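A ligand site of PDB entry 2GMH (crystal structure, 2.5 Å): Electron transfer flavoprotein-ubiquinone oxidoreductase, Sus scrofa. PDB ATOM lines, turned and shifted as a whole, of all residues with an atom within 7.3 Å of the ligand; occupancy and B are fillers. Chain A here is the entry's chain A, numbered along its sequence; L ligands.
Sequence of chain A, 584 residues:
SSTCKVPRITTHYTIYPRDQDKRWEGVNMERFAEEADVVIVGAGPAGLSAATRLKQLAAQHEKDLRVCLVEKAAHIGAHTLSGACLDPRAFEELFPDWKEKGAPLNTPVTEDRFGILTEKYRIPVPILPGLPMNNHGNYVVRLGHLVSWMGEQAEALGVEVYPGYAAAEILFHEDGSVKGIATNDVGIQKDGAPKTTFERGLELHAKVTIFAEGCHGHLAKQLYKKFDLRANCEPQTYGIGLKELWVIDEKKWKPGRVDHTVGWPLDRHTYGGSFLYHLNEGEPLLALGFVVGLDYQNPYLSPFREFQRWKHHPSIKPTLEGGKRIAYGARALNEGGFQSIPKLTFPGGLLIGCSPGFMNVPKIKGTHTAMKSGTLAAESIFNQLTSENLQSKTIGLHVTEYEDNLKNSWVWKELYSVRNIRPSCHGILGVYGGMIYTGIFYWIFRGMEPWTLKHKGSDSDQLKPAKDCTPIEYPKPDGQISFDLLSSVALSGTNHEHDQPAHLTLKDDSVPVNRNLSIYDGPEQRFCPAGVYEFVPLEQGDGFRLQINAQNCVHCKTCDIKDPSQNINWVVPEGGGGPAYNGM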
ATOM      1  N   ILE A 240     -20.250   0.334  30.426  1.00  0.00           N
ATOM      2  CA  ILE A 240     -18.829   0.095  30.682  1.00  0.00           C
ATOM      3  C   ILE A 240     -18.227   1.402  31.191  1.00  0.00           C
ATOM      4  O   ILE A 240     -18.481   2.477  30.632  1.00  0.00           O
ATOM      5  CB  ILE A 240     -18.054  -0.403  29.431  1.00  0.00           C
ATOM      6  CG1 ILE A 240     -16.564  -0.586  29.817  1.00  0.00           C
ATOM      7  CG2 ILE A 240     -18.244   0.555  28.260  1.00  0.00           C
ATOM      8  CD1 ILE A 240     -15.631  -0.928  28.661  1.00  0.00           C
ATOM      9  N   ALA A 330     -10.769  -0.007  33.748  1.00  0.00           N
ATOM     10  CA  ALA A 330     -12.111  -0.099  33.195  1.00  0.00           C
ATOM     11  C   ALA A 330     -12.889  -1.191  33.924  1.00  0.00           C
ATOM     12  O   ALA A 330     -12.317  -2.206  34.283  1.00  0.00           O
ATOM     13  CB  ALA A 330     -12.037  -0.400  31.723  1.00  0.00           C
ATOM     14  N   ALA A 332     -17.159  -2.897  34.073  1.00  0.00           N
ATOM     15  CA  ALA A 332     -18.571  -2.782  33.743  1.00  0.00           C
ATOM     16  C   ALA A 332     -19.388  -2.457  34.998  1.00  0.00           C
ATOM     17  O   ALA A 332     -18.981  -2.793  36.120  1.00  0.00           O
ATOM     18  CB  ALA A 332     -19.055  -4.084  33.106  1.00  0.00           C
ATOM     19  N   HIS A 503      -8.612 -17.227  29.733  1.00  0.00           N
ATOM     20  CA  HIS A 503      -9.790 -17.248  30.583  1.00  0.00           C
ATOM     21  C   HIS A 503     -10.966 -16.633  29.843  1.00  0.00           C
ATOM     22  O   HIS A 503     -12.095 -16.629  30.322  1.00  0.00           O
ATOM     23  CB  HIS A 503      -9.525 -16.521  31.908  1.00  0.00           C
ATOM     24  CG  HIS A 503      -9.055 -15.116  31.744  1.00  0.00           C
ATOM     25  ND1 HIS A 503      -7.751 -14.800  31.450  1.00  0.00           N
ATOM     26  CD2 HIS A 503      -9.719 -13.940  31.806  1.00  0.00           C
ATOM     27  CE1 HIS A 503      -7.628 -13.493  31.332  1.00  0.00           C
ATOM     28  NE2 HIS A 503      -8.819 -12.949  31.547  1.00  0.00           N
ATOM     29  N   LEU A 504     -10.688 -16.103  28.652  1.00  0.00           N
ATOM     30  CA  LEU A 504     -11.738 -15.577  27.818  1.00  0.00           C
ATOM     31  C   LEU A 504     -12.047 -16.802  26.944  1.00  0.00           C
ATOM     32  O   LEU A 504     -11.428 -17.014  25.893  1.00  0.00           O
ATOM     33  CB  LEU A 504     -11.250 -14.427  26.942  1.00  0.00           C
ATOM     34  CG  LEU A 504     -10.850 -13.069  27.549  1.00  0.00           C
ATOM     35  CD1 LEU A 504     -11.894 -12.616  28.571  1.00  0.00           C
ATOM     36  CD2 LEU A 504      -9.471 -13.160  28.179  1.00  0.00           C
ATOM     37  N   GLU A 524     -15.621  -7.094  19.055  1.00  0.00           N
ATOM     38  CA  GLU A 524     -14.720  -7.398  20.143  1.00  0.00           C
ATOM     39  C   GLU A 524     -13.403  -6.626  20.003  1.00  0.00           C
ATOM     40  O   GLU A 524     -12.673  -6.431  20.976  1.00  0.00           O
ATOM     41  CB  GLU A 524     -14.493  -8.909  20.290  1.00  0.00           C
ATOM     42  CG  GLU A 524     -14.120  -9.623  19.016  1.00  0.00           C
ATOM     43  CD  GLU A 524     -15.336 -10.073  18.251  1.00  0.00           C
ATOM     44  OE1 GLU A 524     -15.596 -11.299  18.216  1.00  0.00           O
ATOM     45  OE2 GLU A 524     -16.035  -9.183  17.702  1.00  0.00           O
ATOM     46  N   PHE A 527     -15.002  -3.046  21.603  1.00  0.00           N
ATOM     47  CA  PHE A 527     -15.609  -2.854  22.911  1.00  0.00           C
ATOM     48  C   PHE A 527     -14.718  -3.278  24.081  1.00  0.00           C
ATOM     49  O   PHE A 527     -14.985  -2.928  25.245  1.00  0.00           O
ATOM     50  CB  PHE A 527     -17.014  -3.513  23.000  1.00  0.00           C
ATOM     51  CG  PHE A 527     -17.041  -5.021  22.818  1.00  0.00           C
ATOM     52  CD1 PHE A 527     -16.257  -5.856  23.604  1.00  0.00           C
ATOM     53  CD2 PHE A 527     -17.936  -5.608  21.898  1.00  0.00           C
ATOM     54  CE1 PHE A 527     -16.356  -7.253  23.477  1.00  0.00           C
ATOM     55  CE2 PHE A 527     -18.042  -7.008  21.764  1.00  0.00           C
ATOM     56  CZ  PHE A 527     -17.259  -7.834  22.547  1.00  0.00           C
ATOM     57  N   CYS A 528     -13.632  -4.018  23.795  1.00  0.00           N
ATOM     58  CA  CYS A 528     -12.708  -4.439  24.851  1.00  0.00           C
ATOM     59  C   CYS A 528     -11.793  -3.269  25.182  1.00  0.00           C
ATOM     60  O   CYS A 528     -11.057  -2.805  24.332  1.00  0.00           O
ATOM     61  CB  CYS A 528     -11.864  -5.631  24.420  1.00  0.00           C
ATOM     62  SG  CYS A 528     -10.587  -6.089  25.609  1.00  0.00           S
ATOM     63  N   PRO A 529     -11.819  -2.805  26.420  1.00  0.00           N
ATOM     64  CA  PRO A 529     -10.999  -1.664  26.836  1.00  0.00           C
ATOM     65  C   PRO A 529      -9.518  -2.039  27.030  1.00  0.00           C
ATOM     66  O   PRO A 529      -8.757  -1.262  27.604  1.00  0.00           O
ATOM     67  CB  PRO A 529     -11.635  -1.285  28.164  1.00  0.00           C
ATOM     68  CG  PRO A 529     -11.856  -2.700  28.759  1.00  0.00           C
ATOM     69  CD  PRO A 529     -12.465  -3.440  27.592  1.00  0.00           C
ATOM     70  N   ALA A 530      -9.113  -3.229  26.591  1.00  0.00           N
ATOM     71  CA  ALA A 530      -7.729  -3.630  26.794  1.00  0.00           C
ATOM     72  C   ALA A 530      -6.999  -4.186  25.571  1.00  0.00           C
ATOM     73  O   ALA A 530      -5.849  -4.597  25.691  1.00  0.00           O
ATOM     74  CB  ALA A 530      -7.642  -4.633  27.927  1.00  0.00           C
ATOM     75  N   GLY A 531      -7.666  -4.216  24.424  1.00  0.00           N
ATOM     76  CA  GLY A 531      -7.065  -4.755  23.223  1.00  0.00           C
ATOM     77  C   GLY A 531      -6.791  -6.242  23.309  1.00  0.00           C
ATOM     78  O   GLY A 531      -5.789  -6.700  22.795  1.00  0.00           O
ATOM     79  N   VAL A 532      -7.669  -7.012  23.947  1.00  0.00           N
ATOM     80  CA  VAL A 532      -7.455  -8.452  24.059  1.00  0.00           C
ATOM     81  C   VAL A 532      -7.729  -9.230  22.768  1.00  0.00           C
ATOM     82  O   VAL A 532      -6.952 -10.115  22.372  1.00  0.00           O
ATOM     83  CB  VAL A 532      -8.310  -9.055  25.194  1.00  0.00           C
ATOM     84  CG1 VAL A 532      -8.284 -10.578  25.130  1.00  0.00           C
ATOM     85  CG2 VAL A 532      -7.755  -8.570  26.523  1.00  0.00           C
ATOM     86  N   TYR A 533      -8.830  -8.914  22.104  1.00  0.00           N
ATOM     87  CA  TYR A 533      -9.183  -9.588  20.878  1.00  0.00           C
ATOM     88  C   TYR A 533      -8.684  -8.827  19.649  1.00  0.00           C
ATOM     89  O   TYR A 533      -8.926  -7.639  19.502  1.00  0.00           O
ATOM     90  CB  TYR A 533     -10.712  -9.743  20.799  1.00  0.00           C
ATOM     91  CG  TYR A 533     -11.344 -10.372  21.984  1.00  0.00           C
ATOM     92  CD1 TYR A 533     -11.975  -9.597  22.967  1.00  0.00           C
ATOM     93  CD2 TYR A 533     -11.319 -11.751  22.161  1.00  0.00           C
ATOM     94  CE1 TYR A 533     -12.564 -10.164  24.077  1.00  0.00           C
ATOM     95  CE2 TYR A 533     -11.892 -12.340  23.264  1.00  0.00           C
ATOM     96  CZ  TYR A 533     -12.518 -11.539  24.230  1.00  0.00           C
ATOM     97  OH  TYR A 533     -13.041 -12.122  25.370  1.00  0.00           O
ATOM     98  N   ILE A 548      -6.433 -14.167  20.856  1.00  0.00           N
ATOM     99  CA  ILE A 548      -6.834 -13.716  22.176  1.00  0.00           C
ATOM    100  C   ILE A 548      -5.587 -13.452  23.011  1.00  0.00           C
ATOM    101  O   ILE A 548      -4.819 -14.355  23.308  1.00  0.00           O
ATOM    102  CB  ILE A 548      -7.718 -14.820  22.870  1.00  0.00           C
ATOM    103  CG1 ILE A 548      -9.078 -14.897  22.160  1.00  0.00           C
ATOM    104  CG2 ILE A 548      -7.875 -14.530  24.361  1.00  0.00           C
ATOM    105  CD1 ILE A 548     -10.071 -15.903  22.741  1.00  0.00           C
ATOM    106  N   ASN A 549      -5.367 -12.189  23.379  1.00  0.00           N
ATOM    107  CA  ASN A 549      -4.215 -11.806  24.213  1.00  0.00           C
ATOM    108  C   ASN A 549      -4.712 -11.706  25.648  1.00  0.00           C
ATOM    109  O   ASN A 549      -4.845 -10.607  26.208  1.00  0.00           O
ATOM    110  CB  ASN A 549      -3.644 -10.482  23.748  1.00  0.00           C
ATOM    111  CG  ASN A 549      -3.267 -10.507  22.283  1.00  0.00           C
ATOM    112  OD1 ASN A 549      -2.452 -11.337  21.852  1.00  0.00           O
ATOM    113  ND2 ASN A 549      -3.870  -9.619  21.510  1.00  0.00           N
ATOM    114  N   ALA A 550      -4.983 -12.870  26.208  1.00  0.00           N
ATOM    115  CA  ALA A 550      -5.521 -12.980  27.555  1.00  0.00           C
ATOM    116  C   ALA A 550      -4.717 -12.288  28.660  1.00  0.00           C
ATOM    117  O   ALA A 550      -5.243 -11.920  29.707  1.00  0.00           O
ATOM    118  CB  ALA A 550      -5.734 -14.463  27.881  1.00  0.00           C
ATOM    119  N   ASN A 552      -3.601  -9.323  28.669  1.00  0.00           N
ATOM    120  CA  ASN A 552      -3.944  -7.907  28.782  1.00  0.00           C
ATOM    121  C   ASN A 552      -5.296  -7.655  29.429  1.00  0.00           C
ATOM    122  O   ASN A 552      -5.694  -6.505  29.588  1.00  0.00           O
ATOM    123  CB  ASN A 552      -3.953  -7.283  27.393  1.00  0.00           C
ATOM    124  CG  ASN A 552      -2.574  -7.261  26.757  1.00  0.00           C
ATOM    125  OD1 ASN A 552      -2.453  -7.479  25.549  1.00  0.00           O
ATOM    126  ND2 ASN A 552      -1.533  -7.003  27.537  1.00  0.00           N
ATOM    127  N   CYS A 553      -6.006  -8.693  29.830  1.00  0.00           N
ATOM    128  CA  CYS A 553      -7.337  -8.540  30.408  1.00  0.00           C
ATOM    129  C   CYS A 553      -7.363  -7.729  31.713  1.00  0.00           C
ATOM    130  O   CYS A 553      -6.561  -7.981  32.620  1.00  0.00           O
ATOM    131  CB  CYS A 553      -7.941  -9.924  30.661  1.00  0.00           C
ATOM    132  SG  CYS A 553      -9.702 -10.006  31.117  1.00  0.00           S
ATOM    133  N   VAL A 554      -8.278  -6.768  31.806  1.00  0.00           N
ATOM    134  CA  VAL A 554      -8.407  -6.012  33.046  1.00  0.00           C
ATOM    135  C   VAL A 554      -9.616  -6.514  33.850  1.00  0.00           C
ATOM    136  O   VAL A 554      -9.975  -5.938  34.867  1.00  0.00           O
ATOM    137  CB  VAL A 554      -8.538  -4.475  32.830  1.00  0.00           C
ATOM    138  CG1 VAL A 554      -7.322  -3.955  32.103  1.00  0.00           C
ATOM    139  CG2 VAL A 554      -9.834  -4.137  32.071  1.00  0.00           C
ATOM    140  N   HIS A 555     -10.221  -7.607  33.396  1.00  0.00           N
ATOM    141  CA  HIS A 555     -11.373  -8.227  34.071  1.00  0.00           C
ATOM    142  C   HIS A 555     -12.610  -7.311  34.206  1.00  0.00           C
ATOM    143  O   HIS A 555     -13.340  -7.400  35.195  1.00  0.00           O
ATOM    144  CB  HIS A 555     -10.979  -8.686  35.496  1.00  0.00           C
ATOM    145  CG  HIS A 555      -9.743  -9.542  35.549  1.00  0.00           C
ATOM    146  ND1 HIS A 555      -9.479 -10.391  36.620  1.00  0.00           N
ATOM    147  CD2 HIS A 555      -8.714  -9.702  34.681  1.00  0.00           C
ATOM    148  CE1 HIS A 555      -8.344 -11.032  36.387  1.00  0.00           C
ATOM    149  NE2 HIS A 555      -7.862 -10.633  35.225  1.00  0.00           N
ATOM    150  N   CYS A 556     -12.874  -6.459  33.226  1.00  0.00           N
ATOM    151  CA  CYS A 556     -14.012  -5.544  33.333  1.00  0.00           C
ATOM    152  C   CYS A 556     -15.376  -6.243  33.166  1.00  0.00           C
ATOM    153  O   CYS A 556     -16.396  -5.748  33.697  1.00  0.00           O
ATOM    154  CB  CYS A 556     -13.899  -4.460  32.256  1.00  0.00           C
ATOM    155  SG  CYS A 556     -14.037  -5.078  30.560  1.00  0.00           S
ATOM    156  N   LYS A 557     -15.356  -7.383  32.468  1.00  0.00           N
ATOM    157  CA  LYS A 557     -16.473  -8.260  32.168  1.00  0.00           C
ATOM    158  C   LYS A 557     -17.357  -7.839  30.961  1.00  0.00           C
ATOM    159  O   LYS A 557     -18.433  -8.410  30.750  1.00  0.00           O
ATOM    160  CB  LYS A 557     -17.352  -8.468  33.417  1.00  0.00           C
ATOM    161  CG  LYS A 557     -16.587  -8.994  34.631  1.00  0.00           C
ATOM    162  CD  LYS A 557     -15.733 -10.200  34.304  1.00  0.00           C
ATOM    163  CE  LYS A 557     -15.232 -10.779  35.609  1.00  0.00           C
ATOM    164  NZ  LYS A 557     -16.388 -11.415  36.328  1.00  0.00           N
ATOM    165  N   THR A 558     -16.888  -6.871  30.175  1.00  0.00           N
ATOM    166  CA  THR A 558     -17.643  -6.364  29.021  1.00  0.00           C
ATOM    167  C   THR A 558     -17.891  -7.352  27.877  1.00  0.00           C
ATOM    168  O   THR A 558     -19.005  -7.458  27.348  1.00  0.00           O
ATOM    169  CB  THR A 558     -16.952  -5.152  28.404  1.00  0.00           C
ATOM    170  OG1 THR A 558     -16.874  -4.117  29.369  1.00  0.00           O
ATOM    171  CG2 THR A 558     -17.735  -4.642  27.264  1.00  0.00           C
ATOM    172  N   CYS A 559     -16.846  -8.049  27.460  1.00  0.00           N
ATOM    173  CA  CYS A 559     -16.992  -8.974  26.347  1.00  0.00           C
ATOM    174  C   CYS A 559     -18.017 -10.076  26.653  1.00  0.00           C
ATOM    175  O   CYS A 559     -18.741 -10.496  25.765  1.00  0.00           O
ATOM    176  CB  CYS A 559     -15.634  -9.574  26.027  1.00  0.00           C
ATOM    177  SG  CYS A 559     -14.903 -10.345  27.453  1.00  0.00           S
ATOM    178  N   ASP A 560     -18.097 -10.511  27.910  1.00  0.00           N
ATOM    179  CA  ASP A 560     -19.047 -11.560  28.251  1.00  0.00           C
ATOM    180  C   ASP A 560     -20.444 -10.987  28.195  1.00  0.00           C
ATOM    181  O   ASP A 560     -21.424 -11.697  27.993  1.00  0.00           O
ATOM    182  CB  ASP A 560     -18.745 -12.126  29.639  1.00  0.00           C
ATOM    183  CG  ASP A 560     -19.644 -13.280  30.004  1.00  0.00           C
ATOM    184  OD1 ASP A 560     -20.879 -13.109  30.011  1.00  0.00           O
ATOM    185  OD2 ASP A 560     -19.109 -14.370  30.285  1.00  0.00           O
ATOM    186  N   ILE A 568     -18.907 -15.878  24.208  1.00  0.00           N
ATOM    187  CA  ILE A 568     -17.823 -15.755  25.191  1.00  0.00           C
ATOM    188  C   ILE A 568     -18.288 -16.046  26.637  1.00  0.00           C
ATOM    189  O   ILE A 568     -19.427 -15.760  27.010  1.00  0.00           O
ATOM    190  CB  ILE A 568     -17.203 -14.337  25.167  1.00  0.00           C
ATOM    191  CG1 ILE A 568     -16.646 -14.035  23.787  1.00  0.00           C
ATOM    192  CG2 ILE A 568     -16.047 -14.236  26.160  1.00  0.00           C
ATOM    193  CD1 ILE A 568     -16.281 -12.572  23.599  1.00  0.00           C
ATOM    194  N   TRP A 570     -16.491 -15.461  30.358  1.00  0.00           N
ATOM    195  CA  TRP A 570     -15.350 -15.044  31.141  1.00  0.00           C
ATOM    196  C   TRP A 570     -15.265 -15.924  32.401  1.00  0.00           C
ATOM    197  O   TRP A 570     -16.271 -16.166  33.050  1.00  0.00           O
ATOM    198  CB  TRP A 570     -15.488 -13.569  31.560  1.00  0.00           C
ATOM    199  CG  TRP A 570     -14.221 -12.989  32.118  1.00  0.00           C
ATOM    200  CD1 TRP A 570     -13.329 -12.246  31.431  1.00  0.00           C
ATOM    201  CD2 TRP A 570     -13.715 -13.113  33.464  1.00  0.00           C
ATOM    202  NE1 TRP A 570     -12.281 -11.888  32.250  1.00  0.00           N
ATOM    203  CE2 TRP A 570     -12.495 -12.419  33.510  1.00  0.00           C
ATOM    204  CE3 TRP A 570     -14.156 -13.743  34.630  1.00  0.00           C
ATOM    205  CZ2 TRP A 570     -11.705 -12.317  34.678  1.00  0.00           C
ATOM    206  CZ3 TRP A 570     -13.379 -13.651  35.801  1.00  0.00           C
ATOM    207  CH2 TRP A 570     -12.168 -12.942  35.804  1.00  0.00           C
HETATM  208 FE1  LIG L   1     -10.914  -8.663  29.642  1.00  0.00          FE
HETATM  209 FE2  LIG L   1     -11.383  -7.198  27.379  1.00  0.00          FE
HETATM  210 FE3  LIG L   1     -12.878  -6.726  29.640  1.00  0.00          FE
HETATM  211 FE4  LIG L   1     -13.228  -8.998  28.244  1.00  0.00          FE
HETATM  212  S1  LIG L   1     -13.640  -7.006  27.482  1.00  0.00           S
HETATM  213  S2  LIG L   1     -13.028  -8.881  30.416  1.00  0.00           S
HETATM  214  S3  LIG L   1     -11.227  -9.484  27.506  1.00  0.00           S
HETATM  215  S4  LIG L   1     -10.723  -6.395  29.414  1.00  0.00           S
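N of Cys 556 sits close to S2 of the ligand, at 3.7 Å. The side-chain sulfur (SG) of Cys 556 is bound to an iron atom (FE3) of the ligand (2.2 Å). FE2 of the ligand is bound by SG of Cys 528 (2.2 Å). N of Cys 559 sits close to S1 of the ligand (3.4 Å). The side-chain sulfur (SG) of Cys 559 is bound to an iron atom (FE4) of the ligand, at 2.3 Å. FE1 of the ligand is bound by SG of Cys 553, 2.3 Å away. A sulfur (S4) of the ligand sits close to the backbone NH (N) of Val 554, at 3.4 Å. N of Lys 557 sits close to S2 of the ligand. The indole nitrogen (NE1) of Trp 570 lies close to a sulfur (S2) of the ligand (3.6 Å).
The side-chain sulfur of Cys 556 sits close to the side-chain hydroxyl of Thr 558 (3.2 Å). O of Cys 556 lies within hydrogen-bond range of N of Ala 332 (3.0 Å). The side-chain sulfur (SG) of Cys 528 sits close to the backbone NH (N) of Ala 530. SG of Cys 528 lies close to N of Gly 531 (3.7 Å). SG of Cys 553 sits close to NE1 of Trp 570 (3.4 Å). The side-chain sulfur of Cys 553 sits close to a ring nitrogen (NE2) of His 503. N of Trp 570 sits at hydrogen-bond distance from OD2 of Asp 560 (2.8 Å). The backbone carbonyl oxygen (O) of Val 532 sits at hydrogen-bond distance from the backbone NH (N) of Asn 549 (2.8 Å).
Leu 504 touches the ligand. Pro 529 touches the ligand (CD to S1, 3.8 Å). Ala 530 touches the ligand (CB to S4, 3.8 Å). Val 532 touches the ligand. Tyr 533 touches the ligand (CE1 to S3, 3.7 Å). N of His 555 touches FE1 of the ligand (3.96 Å). Thr 558 touches the ligand (CB to S1, 3.9 Å). Hydrophobic or aromatic side chains within 4 Å of the ligand: Leu 504, Pro 529, Ala 530, Val 532, Tyr 533, Val 554 and Trp 570. 14 residues have an atom within 4 Å of the ligand: Leu 504, Cys 528, Pro 529, Ala 530, Val 532, Tyr 533, Cys 553, Val 554, His 555, Cys 556, Lys 557, Thr 558, Cys 559 and Trp 570. Along chain A the residues within 4 Å of the ligand span positions 504 to 570. The nearest printed residue that does not touch the ligand is Phe 527 (4.8 Å).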
